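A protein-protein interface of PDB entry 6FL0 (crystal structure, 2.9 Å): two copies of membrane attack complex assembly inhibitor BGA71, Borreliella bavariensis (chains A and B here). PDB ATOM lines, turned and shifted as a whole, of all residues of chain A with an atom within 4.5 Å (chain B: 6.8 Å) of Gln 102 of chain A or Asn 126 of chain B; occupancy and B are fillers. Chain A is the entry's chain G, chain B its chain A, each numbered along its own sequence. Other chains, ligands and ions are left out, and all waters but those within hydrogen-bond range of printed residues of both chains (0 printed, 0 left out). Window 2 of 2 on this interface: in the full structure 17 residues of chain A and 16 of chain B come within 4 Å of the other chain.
Of the printed residues of chain A, Asn 126 of chain B touches Glu 57 (2.3 Å), Tyr 101 (3.7 Å) and Gln 102 (3.96 Å). Of the printed residues of chain A, Leu 127 of chain B touches Tyr 101, Gln 102 and Ser 106. Printed residues of chain A within 4 Å of Glu 14 of chain B: Glu 57 (2.7 Å). Of the printed residues of chain B, Tyr 101 of chain A touches Asn 126 and Leu 127. Of the printed residues of chain B, Ser 106 of chain A touches Leu 127. The nearest printed residue of chain A that does not touch Glu 14 of chain B is Tyr 101 of chain A (7.1 Å).
Among the printed residues, pairs that only touch across the chains: Ser 106 of chain A with Leu 127 of chain B, Gln 102 of chain A with Leu 127 of chain B, Glu 57 of chain A with Ile 122 of chain B, Tyr 101 of chain A with Leu 127 of chain B, Tyr 101 of chain A with Asn 126 of chain B and Gln 102 of chain A with Asn 126 of chain B.
Of the 10 printed residues of chain A, 4 touch a printed residue of chain B. Hydrophobic or aromatic side chains of chain A that line the printed part of chain B: Tyr 101.
The side-chain carboxylate of Glu 98 of chain A lies close to the side-chain amide oxygen of Gln 102 of chain A, at 3.4 Å.
OE2 of Glu 57 of chain A lies close to OD1 of Asn 126 of chain B (2.3 Å). The side-chain carboxylate of Glu 57 of chain A lies close to the side-chain carboxylate of Glu 14 of chain B (2.7 Å).
No position is printed for both chains. Of the 8 pairs that touch across the chains among the printed residues, none has its exchanged pair printed and touching as well.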
ATOM      1  N   GLU A  57       4.065 -21.373  -8.716  1.00  0.00           N
ATOM      2  CA  GLU A  57       3.457 -20.707  -7.531  1.00  0.00           C
ATOM      3  C   GLU A  57       1.931 -20.608  -7.703  1.00  0.00           C
ATOM      4  O   GLU A  57       1.168 -20.924  -6.786  1.00  0.00           O
ATOM      5  CB  GLU A  57       4.015 -19.291  -7.324  1.00  0.00           C
ATOM      6  CG  GLU A  57       5.518 -19.222  -7.079  1.00  0.00           C
ATOM      7  CD  GLU A  57       6.066 -17.812  -6.910  1.00  0.00           C
ATOM      8  OE1 GLU A  57       6.334 -17.134  -7.925  1.00  0.00           O
ATOM      9  OE2 GLU A  57       6.209 -17.387  -5.753  1.00  0.00           O
ATOM     10  N   LYS A  97      -2.427  -9.923  -1.452  1.00  0.00           N
ATOM     11  CA  LYS A  97      -1.150 -10.593  -1.727  1.00  0.00           C
ATOM     12  C   LYS A  97      -0.694 -11.459  -0.539  1.00  0.00           C
ATOM     13  O   LYS A  97      -0.347 -12.625  -0.731  1.00  0.00           O
ATOM     14  CB  LYS A  97      -0.063  -9.572  -2.061  1.00  0.00           C
ATOM     15  CG  LYS A  97      -0.014  -9.161  -3.518  1.00  0.00           C
ATOM     16  CD  LYS A  97       0.980  -8.066  -3.779  1.00  0.00           C
ATOM     17  CE  LYS A  97       1.128  -7.783  -5.257  1.00  0.00           C
ATOM     18  NZ  LYS A  97       2.169  -6.762  -5.513  1.00  0.00           N
ATOM     19  N   GLU A  98      -0.652 -10.886   0.669  1.00  0.00           N
ATOM     20  CA  GLU A  98      -0.169 -11.632   1.843  1.00  0.00           C
ATOM     21  C   GLU A  98      -1.008 -12.910   1.994  1.00  0.00           C
ATOM     22  O   GLU A  98      -0.471 -13.986   2.196  1.00  0.00           O
ATOM     23  CB  GLU A  98      -0.131 -10.755   3.104  1.00  0.00           C
ATOM     24  CG  GLU A  98       1.072  -9.818   3.119  1.00  0.00           C
ATOM     25  CD  GLU A  98       1.433  -9.057   4.391  1.00  0.00           C
ATOM     26  OE1 GLU A  98       0.748  -9.203   5.437  1.00  0.00           O
ATOM     27  OE2 GLU A  98       2.420  -8.304   4.320  1.00  0.00           O
ATOM     28  N   PHE A  99      -2.326 -12.799   1.833  1.00  0.00           N
ATOM     29  CA  PHE A  99      -3.197 -13.958   1.902  1.00  0.00           C
ATOM     30  C   PHE A  99      -2.660 -15.063   0.979  1.00  0.00           C
ATOM     31  O   PHE A  99      -2.403 -16.188   1.415  1.00  0.00           O
ATOM     32  CB  PHE A  99      -4.626 -13.554   1.544  1.00  0.00           C
ATOM     33  CG  PHE A  99      -5.616 -14.689   1.505  1.00  0.00           C
ATOM     34  CD1 PHE A  99      -6.192 -15.172   2.671  1.00  0.00           C
ATOM     35  CD2 PHE A  99      -5.993 -15.256   0.299  1.00  0.00           C
ATOM     36  CE1 PHE A  99      -7.117 -16.203   2.633  1.00  0.00           C
ATOM     37  CE2 PHE A  99      -6.914 -16.289   0.263  1.00  0.00           C
ATOM     38  CZ  PHE A  99      -7.469 -16.765   1.428  1.00  0.00           C
ATOM     39  N   ILE A 100      -2.459 -14.714  -0.294  1.00  0.00           N
ATOM     40  CA  ILE A 100      -2.116 -15.665  -1.343  1.00  0.00           C
ATOM     41  C   ILE A 100      -0.686 -16.188  -1.140  1.00  0.00           C
ATOM     42  O   ILE A 100      -0.462 -17.407  -1.126  1.00  0.00           O
ATOM     43  CB  ILE A 100      -2.320 -15.007  -2.726  1.00  0.00           C
ATOM     44  CG1 ILE A 100      -3.807 -14.905  -3.087  1.00  0.00           C
ATOM     45  CG2 ILE A 100      -1.528 -15.721  -3.812  1.00  0.00           C
ATOM     46  CD1 ILE A 100      -4.524 -16.234  -3.224  1.00  0.00           C
ATOM     47  N   TYR A 101       0.270 -15.264  -0.985  1.00  0.00           N
ATOM     48  CA  TYR A 101       1.701 -15.569  -1.048  1.00  0.00           C
ATOM     49  C   TYR A 101       2.293 -15.891   0.331  1.00  0.00           C
ATOM     50  O   TYR A 101       3.434 -16.362   0.384  1.00  0.00           O
ATOM     51  CB  TYR A 101       2.500 -14.381  -1.582  1.00  0.00           C
ATOM     52  CG  TYR A 101       2.389 -14.087  -3.056  1.00  0.00           C
ATOM     53  CD1 TYR A 101       2.672 -15.048  -4.013  1.00  0.00           C
ATOM     54  CD2 TYR A 101       2.068 -12.813  -3.495  1.00  0.00           C
ATOM     55  CE1 TYR A 101       2.602 -14.761  -5.367  1.00  0.00           C
ATOM     56  CE2 TYR A 101       1.997 -12.504  -4.844  1.00  0.00           C
ATOM     57  CZ  TYR A 101       2.266 -13.484  -5.784  1.00  0.00           C
ATOM     58  OH  TYR A 101       2.198 -13.177  -7.113  1.00  0.00           O
ATOM     59  N   GLN A 102       1.562 -15.586   1.419  1.00  0.00           N
ATOM     60  CA  GLN A 102       2.081 -15.759   2.792  1.00  0.00           C
ATOM     61  C   GLN A 102       1.322 -16.889   3.496  1.00  0.00           C
ATOM     62  O   GLN A 102       1.952 -17.848   3.908  1.00  0.00           O
ATOM     63  CB  GLN A 102       2.076 -14.443   3.580  1.00  0.00           C
ATOM     64  CG  GLN A 102       3.035 -13.413   2.995  1.00  0.00           C
ATOM     65  CD  GLN A 102       3.319 -12.220   3.879  1.00  0.00           C
ATOM     66  OE1 GLN A 102       2.671 -11.998   4.906  1.00  0.00           O
ATOM     67  NE2 GLN A 102       4.300 -11.423   3.471  1.00  0.00           N
ATOM     68  N   ILE A 103      -0.008 -16.784   3.608  1.00  0.00           N
ATOM     69  CA  ILE A 103      -0.837 -17.842   4.233  1.00  0.00           C
ATOM     70  C   ILE A 103      -0.952 -19.051   3.287  1.00  0.00           C
ATOM     71  O   ILE A 103      -0.480 -20.132   3.622  1.00  0.00           O
ATOM     72  CB  ILE A 103      -2.228 -17.315   4.634  1.00  0.00           C
ATOM     73  CG1 ILE A 103      -2.146 -16.127   5.596  1.00  0.00           C
ATOM     74  CG2 ILE A 103      -3.084 -18.435   5.205  1.00  0.00           C
ATOM     75  CD1 ILE A 103      -1.558 -16.460   6.955  1.00  0.00           C
ATOM     76  N   VAL A 104      -1.576 -18.863   2.115  1.00  0.00           N
ATOM     77  CA  VAL A 104      -2.058 -19.975   1.280  1.00  0.00           C
ATOM     78  C   VAL A 104      -0.882 -20.816   0.757  1.00  0.00           C
ATOM     79  O   VAL A 104      -0.958 -22.054   0.738  1.00  0.00           O
ATOM     80  CB  VAL A 104      -2.945 -19.473   0.122  1.00  0.00           C
ATOM     81  CG1 VAL A 104      -3.206 -20.557  -0.912  1.00  0.00           C
ATOM     82  CG2 VAL A 104      -4.263 -18.924   0.631  1.00  0.00           C
ATOM     83  N   SER A 106       2.150 -20.952   2.147  1.00  0.00           N
ATOM     84  CA  SER A 106       2.827 -21.573   3.285  1.00  0.00           C
ATOM     85  C   SER A 106       2.123 -22.860   3.751  1.00  0.00           C
ATOM     86  O   SER A 106       2.783 -23.823   4.150  1.00  0.00           O
ATOM     87  CB  SER A 106       2.936 -20.595   4.403  1.00  0.00           C
ATOM     88  OG  SER A 106       3.560 -19.414   3.936  1.00  0.00           O
ATOM     89  N   GLU B  14      12.772 -19.299 -10.752  1.00  0.00           N
ATOM     90  CA  GLU B  14      11.376 -19.597 -11.102  1.00  0.00           C
ATOM     91  C   GLU B  14      11.333 -20.364 -12.432  1.00  0.00           C
ATOM     92  O   GLU B  14      10.712 -21.435 -12.497  1.00  0.00           O
ATOM     93  CB  GLU B  14      10.519 -18.329 -11.151  1.00  0.00           C
ATOM     94  CG  GLU B  14      10.028 -17.874  -9.783  1.00  0.00           C
ATOM     95  CD  GLU B  14       9.382 -16.498  -9.771  1.00  0.00           C
ATOM     96  OE1 GLU B  14       9.559 -15.783 -10.773  1.00  0.00           O
ATOM     97  OE2 GLU B  14       8.690 -16.141  -8.764  1.00  0.00           O
ATOM     98  N   ALA B 121      13.005 -22.106  -1.957  1.00  0.00           N
ATOM     99  CA  ALA B 121      13.632 -20.798  -2.109  1.00  0.00           C
ATOM    100  C   ALA B 121      12.668 -19.821  -2.796  1.00  0.00           C
ATOM    101  O   ALA B 121      12.658 -18.622  -2.508  1.00  0.00           O
ATOM    102  CB  ALA B 121      14.911 -20.941  -2.897  1.00  0.00           C
ATOM    103  N   ILE B 122      11.872 -20.346  -3.728  1.00  0.00           N
ATOM    104  CA  ILE B 122      10.941 -19.532  -4.478  1.00  0.00           C
ATOM    105  C   ILE B 122       9.825 -19.070  -3.534  1.00  0.00           C
ATOM    106  O   ILE B 122       9.453 -17.899  -3.544  1.00  0.00           O
ATOM    107  CB  ILE B 122      10.421 -20.298  -5.714  1.00  0.00           C
ATOM    108  CG1 ILE B 122      11.460 -20.290  -6.841  1.00  0.00           C
ATOM    109  CG2 ILE B 122       9.076 -19.755  -6.184  1.00  0.00           C
ATOM    110  CD1 ILE B 122      11.314 -21.428  -7.828  1.00  0.00           C
ATOM    111  N   ILE B 123       9.315 -19.992  -2.713  1.00  0.00           N
ATOM    112  CA  ILE B 123       8.197 -19.726  -1.837  1.00  0.00           C
ATOM    113  C   ILE B 123       8.671 -18.793  -0.722  1.00  0.00           C
ATOM    114  O   ILE B 123       8.058 -17.748  -0.508  1.00  0.00           O
ATOM    115  CB  ILE B 123       7.589 -21.040  -1.306  1.00  0.00           C
ATOM    116  CG1 ILE B 123       6.961 -21.864  -2.440  1.00  0.00           C
ATOM    117  CG2 ILE B 123       6.596 -20.781  -0.174  1.00  0.00           C
ATOM    118  CD1 ILE B 123       5.787 -21.199  -3.139  1.00  0.00           C
ATOM    119  N   LYS B 124       9.776 -19.163  -0.058  1.00  0.00           N
ATOM    120  CA  LYS B 124      10.417 -18.353   1.004  1.00  0.00           C
ATOM    121  C   LYS B 124      10.761 -16.940   0.513  1.00  0.00           C
ATOM    122  O   LYS B 124      10.939 -16.046   1.326  1.00  0.00           O
ATOM    123  CB  LYS B 124      11.709 -19.003   1.503  1.00  0.00           C
ATOM    124  CG  LYS B 124      11.532 -20.101   2.548  1.00  0.00           C
ATOM    125  CD  LYS B 124      12.813 -20.590   3.215  1.00  0.00           C
ATOM    126  CE  LYS B 124      14.073 -20.233   2.445  1.00  0.00           C
ATOM    127  NZ  LYS B 124      15.115 -21.287   2.513  1.00  0.00           N
ATOM    128  N   ASP B 125      10.913 -16.746  -0.799  1.00  0.00           N
ATOM    129  CA  ASP B 125      11.168 -15.419  -1.320  1.00  0.00           C
ATOM    130  C   ASP B 125       9.953 -14.534  -1.025  1.00  0.00           C
ATOM    131  O   ASP B 125      10.106 -13.395  -0.554  1.00  0.00           O
ATOM    132  CB  ASP B 125      11.488 -15.417  -2.815  1.00  0.00           C
ATOM    133  CG  ASP B 125      12.001 -14.069  -3.292  1.00  0.00           C
ATOM    134  OD1 ASP B 125      12.971 -13.570  -2.685  1.00  0.00           O
ATOM    135  OD2 ASP B 125      11.410 -13.511  -4.241  1.00  0.00           O
ATOM    136  N   ASN B 126       8.760 -15.084  -1.281  1.00  0.00           N
ATOM    137  CA  ASN B 126       7.490 -14.373  -1.120  1.00  0.00           C
ATOM    138  C   ASN B 126       7.250 -14.032   0.360  1.00  0.00           C
ATOM    139  O   ASN B 126       6.566 -13.058   0.662  1.00  0.00           O
ATOM    140  CB  ASN B 126       6.311 -15.175  -1.676  1.00  0.00           C
ATOM    141  CG  ASN B 126       6.380 -15.429  -3.168  1.00  0.00           C
ATOM    142  OD1 ASN B 126       6.150 -16.557  -3.608  1.00  0.00           O
ATOM    143  ND2 ASN B 126       6.651 -14.394  -3.952  1.00  0.00           N
ATOM    144  N   LEU B 127       7.801 -14.847   1.266  1.00  0.00           N
ATOM    145  CA  LEU B 127       7.726 -14.620   2.706  1.00  0.00           C
ATOM    146  C   LEU B 127       8.763 -13.573   3.141  1.00  0.00           C
ATOM    147  O   LEU B 127       8.577 -12.903   4.138  1.00  0.00           O
ATOM    148  CB  LEU B 127       7.955 -15.945   3.444  1.00  0.00           C
ATOM    149  CG  LEU B 127       6.995 -17.089   3.110  1.00  0.00           C
ATOM    150  CD1 LEU B 127       7.363 -18.340   3.894  1.00  0.00           C
ATOM    151  CD2 LEU B 127       5.545 -16.715   3.389  1.00  0.00           C
ATOM    152  N   HIS B 128       9.864 -13.447   2.394  1.00  0.00           N
ATOM    153  CA  HIS B 128      11.012 -12.608   2.781  1.00  0.00           C
ATOM    154  C   HIS B 128      11.839 -13.320   3.865  1.00  0.00           C
ATOM    155  O   HIS B 128      12.177 -12.710   4.888  1.00  0.00           O
ATOM    156  CB  HIS B 128      10.557 -11.207   3.223  1.00  0.00           C
ATOM    157  CG  HIS B 128       9.640 -10.546   2.247  1.00  0.00           C
ATOM    158  ND1 HIS B 128      10.009 -10.324   0.932  1.00  0.00           N
ATOM    159  CD2 HIS B 128       8.382 -10.068   2.375  1.00  0.00           C
ATOM    160  CE1 HIS B 128       9.020  -9.738   0.294  1.00  0.00           C
ATOM    161  NE2 HIS B 128       8.012  -9.569   1.156  1.00  0.00           N
ATOM    162  N   THR B 129      12.151 -14.605   3.630  1.00  0.00           N
ATOM    163  CA  THR B 129      12.987 -15.416   4.521  1.00  0.00           C
ATOM    164  C   THR B 129      13.852 -16.381   3.705  1.00  0.00           C
ATOM    165  O   THR B 129      14.035 -17.511   4.122  1.00  0.00           O
ATOM    166  CB  THR B 129      12.155 -16.221   5.535  1.00  0.00           C
ATOM    167  OG1 THR B 129      11.400 -17.242   4.875  1.00  0.00           O
ATOM    168  CG2 THR B 129      11.227 -15.354   6.358  1.00  0.00           C
ATOM    169  N   GLN B 130      14.378 -15.916   2.562  1.00  0.00           N
ATOM    170  CA  GLN B 130      15.184 -16.735   1.627  1.00  0.00           C
ATOM    171  C   GLN B 130      16.656 -16.710   2.064  1.00  0.00           C
ATOM    172  O   GLN B 130      17.347 -15.709   1.888  1.00  0.00           O
ATOM    173  CB  GLN B 130      15.039 -16.250   0.175  1.00  0.00           C
ATOM    174  CG  GLN B 130      15.361 -17.330  -0.857  1.00  0.00           C
ATOM    175  CD  GLN B 130      15.838 -16.798  -2.189  1.00  0.00           C
ATOM    176  OE1 GLN B 130      15.174 -15.986  -2.826  1.00  0.00           O
ATOM    177  NE2 GLN B 130      16.987 -17.281  -2.641  1.00  0.00           N
